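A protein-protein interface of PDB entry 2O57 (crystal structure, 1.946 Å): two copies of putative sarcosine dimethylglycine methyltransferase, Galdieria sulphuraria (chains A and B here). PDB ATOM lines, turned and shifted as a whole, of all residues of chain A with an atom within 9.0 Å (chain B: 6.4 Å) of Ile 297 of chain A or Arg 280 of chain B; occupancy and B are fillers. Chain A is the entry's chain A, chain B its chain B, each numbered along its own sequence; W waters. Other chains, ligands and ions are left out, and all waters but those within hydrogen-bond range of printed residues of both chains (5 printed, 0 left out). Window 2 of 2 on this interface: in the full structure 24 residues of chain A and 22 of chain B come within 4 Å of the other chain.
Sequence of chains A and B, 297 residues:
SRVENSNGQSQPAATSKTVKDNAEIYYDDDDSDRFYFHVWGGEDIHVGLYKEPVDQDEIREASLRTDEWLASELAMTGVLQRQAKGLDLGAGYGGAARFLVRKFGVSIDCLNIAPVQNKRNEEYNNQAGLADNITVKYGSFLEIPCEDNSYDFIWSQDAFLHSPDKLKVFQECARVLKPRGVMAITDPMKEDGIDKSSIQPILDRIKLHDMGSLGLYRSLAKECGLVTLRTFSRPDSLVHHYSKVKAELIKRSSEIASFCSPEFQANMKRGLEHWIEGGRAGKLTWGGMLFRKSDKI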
ATOM      1  N   ARG A 180      21.831  25.441 -14.121  1.00  0.00           N
ATOM      2  CA  ARG A 180      23.246  25.133 -13.852  1.00  0.00           C
ATOM      3  C   ARG A 180      23.941  26.179 -12.977  1.00  0.00           C
ATOM      4  O   ARG A 180      25.124  26.081 -12.747  1.00  0.00           O
ATOM      5  CB  ARG A 180      24.042  24.822 -15.120  1.00  0.00           C
ATOM      6  CG  ARG A 180      23.435  23.678 -15.972  1.00  0.00           C
ATOM      7  CD  ARG A 180      24.450  23.113 -17.004  1.00  0.00           C
ATOM      8  NE  ARG A 180      25.645  22.542 -16.346  1.00  0.00           N
ATOM      9  CZ  ARG A 180      25.686  21.383 -15.670  1.00  0.00           C
ATOM     10  NH1 ARG A 180      24.594  20.630 -15.490  1.00  0.00           N
ATOM     11  NH2 ARG A 180      26.832  20.981 -15.135  1.00  0.00           N
ATOM     12  N   LYS A 222      16.820  18.907  -3.186  1.00  0.00           N
ATOM     13  CA  LYS A 222      16.558  17.941  -4.270  1.00  0.00           C
ATOM     14  C   LYS A 222      15.144  18.059  -4.790  1.00  0.00           C
ATOM     15  O   LYS A 222      14.927  18.037  -5.981  1.00  0.00           O
ATOM     16  CB  LYS A 222      16.820  16.507  -3.825  1.00  0.00           C
ATOM     17  CG  LYS A 222      16.502  15.424  -4.879  1.00  0.00           C
ATOM     18  CD  LYS A 222      16.797  14.054  -4.287  1.00  0.00           C
ATOM     19  CE  LYS A 222      16.221  12.899  -5.155  1.00  0.00           C
ATOM     20  NZ  LYS A 222      16.824  11.610  -4.710  1.00  0.00           N
ATOM     21  N   LEU A 226      17.617  21.050  -7.086  1.00  0.00           N
ATOM     22  CA  LEU A 226      19.012  21.355  -6.764  1.00  0.00           C
ATOM     23  C   LEU A 226      19.738  20.130  -6.278  1.00  0.00           C
ATOM     24  O   LEU A 226      19.444  19.604  -5.186  1.00  0.00           O
ATOM     25  CB  LEU A 226      19.152  22.460  -5.702  1.00  0.00           C
ATOM     26  CG  LEU A 226      18.410  23.776  -5.920  1.00  0.00           C
ATOM     27  CD1 LEU A 226      18.493  24.678  -4.675  1.00  0.00           C
ATOM     28  CD2 LEU A 226      19.000  24.459  -7.113  1.00  0.00           C
ATOM     29  N   VAL A 227      20.706  19.693  -7.068  1.00  0.00           N
ATOM     30  CA  VAL A 227      21.544  18.544  -6.696  1.00  0.00           C
ATOM     31  C   VAL A 227      22.659  18.993  -5.739  1.00  0.00           C
ATOM     32  O   VAL A 227      23.198  20.107  -5.879  1.00  0.00           O
ATOM     33  CB  VAL A 227      22.097  17.827  -7.952  1.00  0.00           C
ATOM     34  CG1 VAL A 227      23.112  18.685  -8.673  1.00  0.00           C
ATOM     35  CG2 VAL A 227      22.704  16.467  -7.589  1.00  0.00           C
ATOM     36  N   THR A 228      22.971  18.141  -4.763  1.00  0.00           N
ATOM     37  CA  THR A 228      23.999  18.434  -3.785  1.00  0.00           C
ATOM     38  C   THR A 228      25.324  17.936  -4.369  1.00  0.00           C
ATOM     39  O   THR A 228      25.493  16.729  -4.662  1.00  0.00           O
ATOM     40  CB  THR A 228      23.711  17.763  -2.435  1.00  0.00           C
ATOM     41  OG1 THR A 228      22.509  18.309  -1.880  1.00  0.00           O
ATOM     42  CG2 THR A 228      24.860  18.042  -1.486  1.00  0.00           C
ATOM     43  N   LEU A 229      26.220  18.874  -4.603  1.00  0.00           N
ATOM     44  CA  LEU A 229      27.551  18.601  -5.169  1.00  0.00           C
ATOM     45  C   LEU A 229      28.524  18.103  -4.121  1.00  0.00           C
ATOM     46  O   LEU A 229      29.292  17.183  -4.387  1.00  0.00           O
ATOM     47  CB  LEU A 229      28.143  19.861  -5.773  1.00  0.00           C
ATOM     48  CG  LEU A 229      27.427  20.525  -6.960  1.00  0.00           C
ATOM     49  CD1 LEU A 229      28.247  21.733  -7.487  1.00  0.00           C
ATOM     50  CD2 LEU A 229      27.180  19.533  -8.100  1.00  0.00           C
ATOM     51  N   ARG A 230      28.483  18.717  -2.938  1.00  0.00           N
ATOM     52  CA  ARG A 230      29.375  18.378  -1.832  1.00  0.00           C
ATOM     53  C   ARG A 230      28.848  18.952  -0.516  1.00  0.00           C
ATOM     54  O   ARG A 230      28.132  19.971  -0.519  1.00  0.00           O
ATOM     55  CB  ARG A 230      30.789  18.887  -2.117  1.00  0.00           C
ATOM     56  CG  ARG A 230      30.912  20.415  -2.307  1.00  0.00           C
ATOM     57  CD  ARG A 230      32.277  20.831  -2.831  1.00  0.00           C
ATOM     58  NE  ARG A 230      32.332  20.731  -4.300  1.00  0.00           N
ATOM     59  CZ  ARG A 230      32.952  21.593  -5.106  1.00  0.00           C
ATOM     60  NH1 ARG A 230      33.635  22.639  -4.629  1.00  0.00           N
ATOM     61  NH2 ARG A 230      32.907  21.409  -6.416  1.00  0.00           N
ATOM     62  N   LEU A 290      27.321  22.819  -1.261  1.00  0.00           N
ATOM     63  CA  LEU A 290      27.185  23.415  -2.582  1.00  0.00           C
ATOM     64  C   LEU A 290      26.179  22.612  -3.373  1.00  0.00           C
ATOM     65  O   LEU A 290      26.151  21.364  -3.319  1.00  0.00           O
ATOM     66  CB  LEU A 290      28.507  23.469  -3.321  1.00  0.00           C
ATOM     67  CG  LEU A 290      29.413  24.669  -3.017  1.00  0.00           C
ATOM     68  CD1 LEU A 290      30.217  24.379  -1.677  1.00  0.00           C
ATOM     69  CD2 LEU A 290      30.319  24.727  -4.191  1.00  0.00           C
ATOM     70  N   PHE A 291      25.342  23.338  -4.096  1.00  0.00           N
ATOM     71  CA  PHE A 291      24.288  22.743  -4.904  1.00  0.00           C
ATOM     72  C   PHE A 291      24.420  23.255  -6.314  1.00  0.00           C
ATOM     73  O   PHE A 291      24.974  24.337  -6.531  1.00  0.00           O
ATOM     74  CB  PHE A 291      22.908  23.183  -4.412  1.00  0.00           C
ATOM     75  CG  PHE A 291      22.643  22.926  -2.952  1.00  0.00           C
ATOM     76  CD1 PHE A 291      22.157  21.692  -2.525  1.00  0.00           C
ATOM     77  CD2 PHE A 291      22.834  23.938  -2.014  1.00  0.00           C
ATOM     78  CE1 PHE A 291      21.877  21.463  -1.169  1.00  0.00           C
ATOM     79  CE2 PHE A 291      22.546  23.725  -0.662  1.00  0.00           C
ATOM     80  CZ  PHE A 291      22.071  22.486  -0.242  1.00  0.00           C
ATOM     81  N   ARG A 292      23.906  22.496  -7.273  1.00  0.00           N
ATOM     82  CA  ARG A 292      23.733  23.034  -8.607  1.00  0.00           C
ATOM     83  C   ARG A 292      22.287  22.842  -9.066  1.00  0.00           C
ATOM     84  O   ARG A 292      21.667  21.817  -8.775  1.00  0.00           O
ATOM     85  CB  ARG A 292      24.708  22.397  -9.601  1.00  0.00           C
ATOM     86  CG  ARG A 292      24.668  23.037 -10.997  1.00  0.00           C
ATOM     87  CD  ARG A 292      25.562  22.358 -12.037  1.00  0.00           C
ATOM     88  NE  ARG A 292      27.004  22.444 -11.795  1.00  0.00           N
ATOM     89  CZ  ARG A 292      27.810  23.468 -12.109  1.00  0.00           C
ATOM     90  NH1 ARG A 292      27.351  24.613 -12.663  1.00  0.00           N
ATOM     91  NH2 ARG A 292      29.101  23.340 -11.849  1.00  0.00           N
ATOM     92  N   LYS A 293      21.742  23.837  -9.758  1.00  0.00           N
ATOM     93  CA  LYS A 293      20.423  23.715 -10.369  1.00  0.00           C
ATOM     94  C   LYS A 293      20.477  22.833 -11.651  1.00  0.00           C
ATOM     95  O   LYS A 293      20.665  23.332 -12.776  1.00  0.00           O
ATOM     96  CB  LYS A 293      19.834  25.087 -10.696  1.00  0.00           C
ATOM     97  CG  LYS A 293      18.403  25.021 -11.211  1.00  0.00           C
ATOM     98  CD  LYS A 293      17.762  26.438 -11.296  1.00  0.00           C
ATOM     99  CE  LYS A 293      16.445  26.424 -12.075  1.00  0.00           C
ATOM    100  NZ  LYS A 293      15.843  27.814 -12.120  1.00  0.00           N
ATOM    101  N   SER A 294      20.357  21.526 -11.440  1.00  0.00           N
ATOM    102  CA  SER A 294      20.388  20.508 -12.505  1.00  0.00           C
ATOM    103  C   SER A 294      19.884  19.221 -11.885  1.00  0.00           C
ATOM    104  O   SER A 294      19.948  19.039 -10.657  1.00  0.00           O
ATOM    105  CB  SER A 294      21.810  20.276 -13.067  1.00  0.00           C
ATOM    106  OG  SER A 294      22.697  19.877 -12.034  1.00  0.00           O
ATOM    107  N   ASP A 295      19.438  18.326 -12.748  1.00  0.00           N
ATOM    108  CA  ASP A 295      18.905  17.031 -12.356  1.00  0.00           C
ATOM    109  C   ASP A 295      19.998  16.143 -11.766  1.00  0.00           C
ATOM    110  O   ASP A 295      19.738  15.388 -10.832  1.00  0.00           O
ATOM    111  CB  ASP A 295      18.263  16.376 -13.591  1.00  0.00           C
ATOM    112  CG  ASP A 295      17.497  15.095 -13.268  1.00  0.00           C
ATOM    113  OD1 ASP A 295      16.930  14.984 -12.152  1.00  0.00           O
ATOM    114  OD2 ASP A 295      17.446  14.202 -14.159  1.00  0.00           O
ATOM    115  N   LYS A 296      21.220  16.258 -12.287  1.00  0.00           N
ATOM    116  CA  LYS A 296      22.312  15.348 -11.915  1.00  0.00           C
ATOM    117  C   LYS A 296      23.682  15.989 -11.716  1.00  0.00           C
ATOM    118  O   LYS A 296      23.951  17.052 -12.289  1.00  0.00           O
ATOM    119  CB  LYS A 296      22.471  14.222 -12.964  1.00  0.00           C
ATOM    120  CG  LYS A 296      21.298  13.253 -13.094  1.00  0.00           C
ATOM    121  CD  LYS A 296      21.174  12.287 -11.908  1.00  0.00           C
ATOM    122  CE  LYS A 296      20.134  11.196 -12.212  1.00  0.00           C
ATOM    123  NZ  LYS A 296      20.487   9.867 -11.585  1.00  0.00           N
ATOM    124  N   ILE A 297      24.423  15.324 -10.797  1.00  0.00           N
ATOM    125  CA  ILE A 297      25.900  15.293 -10.550  1.00  0.00           C
ATOM    126  C   ILE A 297      26.271  15.303  -9.051  1.00  0.00           C
ATOM    127  O   ILE A 297      27.054  14.476  -8.576  1.00  0.00           O
ATOM    128  CB  ILE A 297      26.798  16.278 -11.361  1.00  0.00           C
ATOM    129  CG1 ILE A 297      26.673  16.031 -12.865  1.00  0.00           C
ATOM    130  CG2 ILE A 297      28.294  16.044 -10.986  1.00  0.00           C
ATOM    131  CD1 ILE A 297      27.128  17.200 -13.713  1.00  0.00           C
ATOM    132  OXT ILE A 297      25.817  16.129  -8.276  1.00  0.00           O
ATOM    133  N   GLU B  52      36.240  23.122 -12.987  1.00  0.00           N
ATOM    134  CA  GLU B  52      35.515  23.276 -14.251  1.00  0.00           C
ATOM    135  C   GLU B  52      36.285  24.157 -15.239  1.00  0.00           C
ATOM    136  O   GLU B  52      36.942  25.121 -14.837  1.00  0.00           O
ATOM    137  CB  GLU B  52      34.121  23.825 -14.031  1.00  0.00           C
ATOM    138  CG  GLU B  52      33.253  22.904 -13.185  1.00  0.00           C
ATOM    139  CD  GLU B  52      32.603  21.783 -13.982  1.00  0.00           C
ATOM    140  OE1 GLU B  52      32.933  21.585 -15.182  1.00  0.00           O
ATOM    141  OE2 GLU B  52      31.751  21.078 -13.400  1.00  0.00           O
ATOM    142  N   PRO B 235      30.472  13.836  -3.575  1.00  0.00           N
ATOM    143  CA  PRO B 235      30.050  12.958  -4.644  1.00  0.00           C
ATOM    144  C   PRO B 235      30.370  13.541  -6.038  1.00  0.00           C
ATOM    145  O   PRO B 235      30.618  12.774  -6.969  1.00  0.00           O
ATOM    146  CB  PRO B 235      28.541  12.827  -4.423  1.00  0.00           C
ATOM    147  CG  PRO B 235      28.161  14.089  -3.667  1.00  0.00           C
ATOM    148  CD  PRO B 235      29.319  14.344  -2.783  1.00  0.00           C
ATOM    149  N   ASP B 236      30.454  14.865  -6.165  1.00  0.00           N
ATOM    150  CA  ASP B 236      30.913  15.431  -7.448  1.00  0.00           C
ATOM    151  C   ASP B 236      32.353  14.954  -7.803  1.00  0.00           C
ATOM    152  O   ASP B 236      32.627  14.550  -8.962  1.00  0.00           O
ATOM    153  CB  ASP B 236      30.779  16.948  -7.471  1.00  0.00           C
ATOM    154  CG  ASP B 236      31.598  17.663  -6.361  1.00  0.00           C
ATOM    155  OD1 ASP B 236      32.209  17.029  -5.438  1.00  0.00           O
ATOM    156  OD2 ASP B 236      31.614  18.889  -6.447  1.00  0.00           O
ATOM    157  N   LEU B 238      33.821  12.204  -6.812  1.00  0.00           N
ATOM    158  CA  LEU B 238      33.688  10.793  -7.129  1.00  0.00           C
ATOM    159  C   LEU B 238      33.328  10.590  -8.623  1.00  0.00           C
ATOM    160  O   LEU B 238      33.966   9.772  -9.326  1.00  0.00           O
ATOM    161  CB  LEU B 238      32.609  10.157  -6.232  1.00  0.00           C
ATOM    162  CG  LEU B 238      32.442   8.656  -6.383  1.00  0.00           C
ATOM    163  CD1 LEU B 238      33.619   7.961  -5.652  1.00  0.00           C
ATOM    164  CD2 LEU B 238      31.077   8.202  -5.811  1.00  0.00           C
ATOM    165  N   VAL B 239      32.311  11.332  -9.085  1.00  0.00           N
ATOM    166  CA  VAL B 239      31.784  11.265 -10.443  1.00  0.00           C
ATOM    167  C   VAL B 239      32.801  11.754 -11.446  1.00  0.00           C
ATOM    168  O   VAL B 239      33.059  11.069 -12.433  1.00  0.00           O
ATOM    169  CB  VAL B 239      30.432  12.059 -10.602  1.00  0.00           C
ATOM    170  CG1 VAL B 239      30.067  12.288 -12.097  1.00  0.00           C
ATOM    171  CG2 VAL B 239      29.293  11.295  -9.902  1.00  0.00           C
ATOM    172  N   HIS B 240      33.388  12.925 -11.191  1.00  0.00           N
ATOM    173  CA  HIS B 240      34.430  13.464 -12.056  1.00  0.00           C
ATOM    174  C   HIS B 240      35.644  12.535 -12.151  1.00  0.00           C
ATOM    175  O   HIS B 240      36.140  12.268 -13.255  1.00  0.00           O
ATOM    176  CB  HIS B 240      34.892  14.831 -11.534  1.00  0.00           C
ATOM    177  CG  HIS B 240      33.819  15.875 -11.555  1.00  0.00           C
ATOM    178  ND1 HIS B 240      33.714  16.859 -10.590  1.00  0.00           N
ATOM    179  CD2 HIS B 240      32.822  16.109 -12.441  1.00  0.00           C
ATOM    180  CE1 HIS B 240      32.693  17.645 -10.877  1.00  0.00           C
ATOM    181  NE2 HIS B 240      32.135  17.214 -11.993  1.00  0.00           N
ATOM    182  N   SER B 243      35.012   9.115 -13.913  1.00  0.00           N
ATOM    183  CA  SER B 243      34.759   9.384 -15.338  1.00  0.00           C
ATOM    184  C   SER B 243      36.060   9.518 -16.069  1.00  0.00           C
ATOM    185  O   SER B 243      36.237   8.953 -17.164  1.00  0.00           O
ATOM    186  CB  SER B 243      33.941  10.678 -15.559  1.00  0.00           C
ATOM    187  OG  SER B 243      32.672  10.531 -14.990  1.00  0.00           O
ATOM    188  N   TRP B 275      30.556   3.261 -10.058  1.00  0.00           N
ATOM    189  CA  TRP B 275      30.968   4.393  -9.199  1.00  0.00           C
ATOM    190  C   TRP B 275      30.291   5.663  -9.679  1.00  0.00           C
ATOM    191  O   TRP B 275      29.716   6.432  -8.880  1.00  0.00           O
ATOM    192  CB  TRP B 275      32.485   4.618  -9.206  1.00  0.00           C
ATOM    193  CG  TRP B 275      33.246   3.733  -8.272  1.00  0.00           C
ATOM    194  CD1 TRP B 275      34.209   2.800  -8.637  1.00  0.00           C
ATOM    195  CD2 TRP B 275      33.143   3.661  -6.833  1.00  0.00           C
ATOM    196  NE1 TRP B 275      34.704   2.167  -7.513  1.00  0.00           N
ATOM    197  CE2 TRP B 275      34.061   2.663  -6.398  1.00  0.00           C
ATOM    198  CE3 TRP B 275      32.369   4.342  -5.860  1.00  0.00           C
ATOM    199  CZ2 TRP B 275      34.227   2.324  -5.031  1.00  0.00           C
ATOM    200  CZ3 TRP B 275      32.524   3.989  -4.511  1.00  0.00           C
ATOM    201  CH2 TRP B 275      33.456   3.001  -4.112  1.00  0.00           C
ATOM    202  N   ILE B 276      30.366   5.880 -10.987  1.00  0.00           N
ATOM    203  CA  ILE B 276      29.805   7.100 -11.620  1.00  0.00           C
ATOM    204  C   ILE B 276      28.275   7.200 -11.419  1.00  0.00           C
ATOM    205  O   ILE B 276      27.727   8.267 -11.012  1.00  0.00           O
ATOM    206  CB  ILE B 276      30.219   7.197 -13.126  1.00  0.00           C
ATOM    207  CG1 ILE B 276      31.765   7.236 -13.267  1.00  0.00           C
ATOM    208  CG2 ILE B 276      29.550   8.412 -13.817  1.00  0.00           C
ATOM    209  CD1 ILE B 276      32.288   6.746 -14.631  1.00  0.00           C
ATOM    210  N   GLU B 277      27.575   6.095 -11.668  1.00  0.00           N
ATOM    211  CA  GLU B 277      26.111   6.078 -11.535  1.00  0.00           C
ATOM    212  C   GLU B 277      25.676   6.131 -10.074  1.00  0.00           C
ATOM    213  O   GLU B 277      24.783   6.896  -9.724  1.00  0.00           O
ATOM    214  CB  GLU B 277      25.508   4.837 -12.157  1.00  0.00           C
ATOM    215  CG  GLU B 277      25.750   4.612 -13.608  1.00  0.00           C
ATOM    216  CD  GLU B 277      25.493   3.135 -13.976  1.00  0.00           C
ATOM    217  OE1 GLU B 277      25.270   2.288 -13.041  1.00  0.00           O
ATOM    218  OE2 GLU B 277      25.529   2.824 -15.189  1.00  0.00           O
ATOM    219  N   GLY B 278      26.278   5.302  -9.224  1.00  0.00           N
ATOM    220  CA  GLY B 278      26.058   5.385  -7.774  1.00  0.00           C
ATOM    221  C   GLY B 278      26.260   6.780  -7.200  1.00  0.00           C
ATOM    222  O   GLY B 278      25.523   7.223  -6.316  1.00  0.00           O
ATOM    223  N   GLY B 279      27.274   7.478  -7.701  1.00  0.00           N
ATOM    224  CA  GLY B 279      27.511   8.852  -7.319  1.00  0.00           C
ATOM    225  C   GLY B 279      26.381   9.781  -7.757  1.00  0.00           C
ATOM    226  O   GLY B 279      25.927  10.623  -6.973  1.00  0.00           O
ATOM    227  N   ARG B 280      25.939   9.659  -9.003  1.00  0.00           N
ATOM    228  CA  ARG B 280      24.836  10.497  -9.504  1.00  0.00           C
ATOM    229  C   ARG B 280      23.482  10.154  -8.876  1.00  0.00           C
ATOM    230  O   ARG B 280      22.579  11.008  -8.823  1.00  0.00           O
ATOM    231  CB  ARG B 280      24.753  10.445 -11.034  1.00  0.00           C
ATOM    232  CG  ARG B 280      25.960  11.009 -11.741  1.00  0.00           C
ATOM    233  CD  ARG B 280      25.664  11.415 -13.181  1.00  0.00           C
ATOM    234  NE  ARG B 280      26.649  10.879 -14.098  1.00  0.00           N
ATOM    235  CZ  ARG B 280      27.607  11.563 -14.726  1.00  0.00           C
ATOM    236  NH1 ARG B 280      27.771  12.867 -14.567  1.00  0.00           N
ATOM    237  NH2 ARG B 280      28.418  10.914 -15.535  1.00  0.00           N
ATOM    238  N   ALA B 281      23.344   8.916  -8.397  1.00  0.00           N
ATOM    239  CA  ALA B 281      22.098   8.403  -7.809  1.00  0.00           C
ATOM    240  C   ALA B 281      21.986   8.673  -6.315  1.00  0.00           C
ATOM    241  O   ALA B 281      20.943   8.401  -5.713  1.00  0.00           O
ATOM    242  CB  ALA B 281      21.966   6.868  -8.089  1.00  0.00           C
ATOM    243  N   GLY B 282      23.036   9.220  -5.704  1.00  0.00           N
ATOM    244  CA  GLY B 282      23.005   9.521  -4.249  1.00  0.00           C
ATOM    245  C   GLY B 282      23.285   8.309  -3.351  1.00  0.00           C
ATOM    246  O   GLY B 282      22.983   8.326  -2.149  1.00  0.00           O
ATOM    247  N   LYS B 283      23.850   7.255  -3.934  1.00  0.00           N
ATOM    248  CA  LYS B 283      24.169   6.040  -3.199  1.00  0.00           C
ATOM    249  C   LYS B 283      25.636   6.038  -2.701  1.00  0.00           C
ATOM    250  O   LYS B 283      25.919   5.447  -1.672  1.00  0.00           O
ATOM    251  CB  LYS B 283      23.985   4.787  -4.067  1.00  0.00           C
ATOM    252  CG  LYS B 283      22.561   4.507  -4.637  1.00  0.00           C
ATOM    253  CD  LYS B 283      22.663   3.150  -5.393  1.00  0.00           C
ATOM    254  CE  LYS B 283      21.349   2.640  -5.933  1.00  0.00           C
ATOM    255  NZ  LYS B 283      21.571   1.443  -6.820  1.00  0.00           N
ATOM    256  N   LEU B 284      26.526   6.697  -3.453  1.00  0.00           N
ATOM    257  CA  LEU B 284      27.982   6.592  -3.232  1.00  0.00           C
ATOM    258  C   LEU B 284      28.610   7.990  -3.152  1.00  0.00           C
ATOM    259  O   LEU B 284      28.117   8.950  -3.785  1.00  0.00           O
ATOM    260  CB  LEU B 284      28.643   5.805  -4.373  1.00  0.00           C
ATOM    261  CG  LEU B 284      28.142   4.382  -4.626  1.00  0.00           C
ATOM    262  CD1 LEU B 284      28.826   3.814  -5.915  1.00  0.00           C
ATOM    263  CD2 LEU B 284      28.407   3.508  -3.402  1.00  0.00           C
HETATM  264  O   HOH W   1      31.496  21.462 -10.949  1.00  0.00           O
HETATM  265  O   HOH W   2      29.099  22.350 -15.222  1.00  0.00           O
HETATM  266  O   HOH W   3      34.633  18.201  -4.807  1.00  0.00           O
HETATM  267  O   HOH W   4      23.170  13.471  -9.166  1.00  0.00           O
HETATM  268  O   HOH W   5      22.898   7.378 -11.851  1.00  0.00           O
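The backbone carbonyl oxygen (O) of Leu 229 of chain A sits close to the backbone NH (N) of Asp 236 of chain B, at 3.1 Å. NH2 of Arg 292 of chain A is in salt-bridge range of OE2 of Glu 52 of chain B (3.8 Å). The guanidinium group of Arg 230 of chain A is in salt-bridge range of the side-chain carboxylate of Asp 236 of chain B, 2.8 Å away.
N of Arg 292 of chain A lies within hydrogen-bond range of O of Val 227 of chain A (2.9 Å). N of Leu 290 of chain A sits at hydrogen-bond distance from O of Arg 230 of chain A (3.1 Å). O of Arg 180 of chain A is in hydrogen-bond range of NH1 of Arg 292 of chain A, 2.7 Å away. The backbone carbonyl oxygen (O) of Asp 236 of chain B lies within hydrogen-bond range of a ring nitrogen (ND1) of His 240 of chain B. OG of Ser 294 of chain A is in hydrogen-bond range of O of Lys 296 of chain A, 3.1 Å away. The backbone NH of Leu 229 of chain A sits at hydrogen-bond distance from the backbone carbonyl oxygen of Leu 290 of chain A (2.8 Å).
Among the printed residues, merely in contact across the chains: Thr 228 of chain A with Pro 235 of chain B (3.9 Å), Leu 229 of chain A with Pro 235 of chain B (3.3 Å), Lys 296 of chain A with Arg 280 of chain B (3.6 Å) and Ile 297 of chain A with Arg 280 of chain B (3.8 Å).
Leu 290 of chain A touches none of the printed residues of chain B. Printed residues of chain B within 4 Å of Ile 297 of chain A: Arg 280. Of the printed residues of chain A, Glu 52 of chain B touches Arg 292 (3.8 Å). Of the printed residues of chain A, Asp 236 of chain B touches Leu 229 and Arg 230. Ser 243 of chain B touches none of the printed residues of chain A. No residue of chain A comes within 4 Å of Gly 278 of chain B. No residue of chain A comes within 4 Å of Gly 279 of chain B. The nearest printed residue of chain B that does not touch Ile 297 of chain A is Val 239 of chain B (4.1 Å). The nearest printed residue of chain A that does not touch Arg 280 of chain B is Asp 295 of chain A (5.6 Å). The nearest printed residue of chain B that does not touch Thr 228 of chain A is Asp 236 of chain B (5.5 Å).
Of the 17 printed residues of chain B, 4 touch a printed residue of chain A. Printed residues of chain B that touch a printed residue of chain A: Glu 52, Pro 235, Asp 236 and Arg 280.
No position is printed for both chains. Of the 7 pairs that touch across the chains among the printed residues, none has its exchanged pair printed and touching as well.
Water W1 bridges the side-chain carboxylate (OE2) of Glu 52 of chain B and the guanidinium group (NH2) of Arg 292 of chain A. Water W4 lies within hydrogen-bond range of O of Arg 280 of chain B (2.6 Å) and N of Ile 297 of chain A (2.8 Å). Water W2 bridges the guanidinium group (NH2) of Arg 180 of chain A and the side-chain carboxylate (OE2) of Glu 52 of chain B. Water W3 bridges OD1 of Asp 236 of chain B and NE of Arg 230 of chain A. Water W5 bridges O of Glu 277 of chain B and NZ of Lys 296 of chain A.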
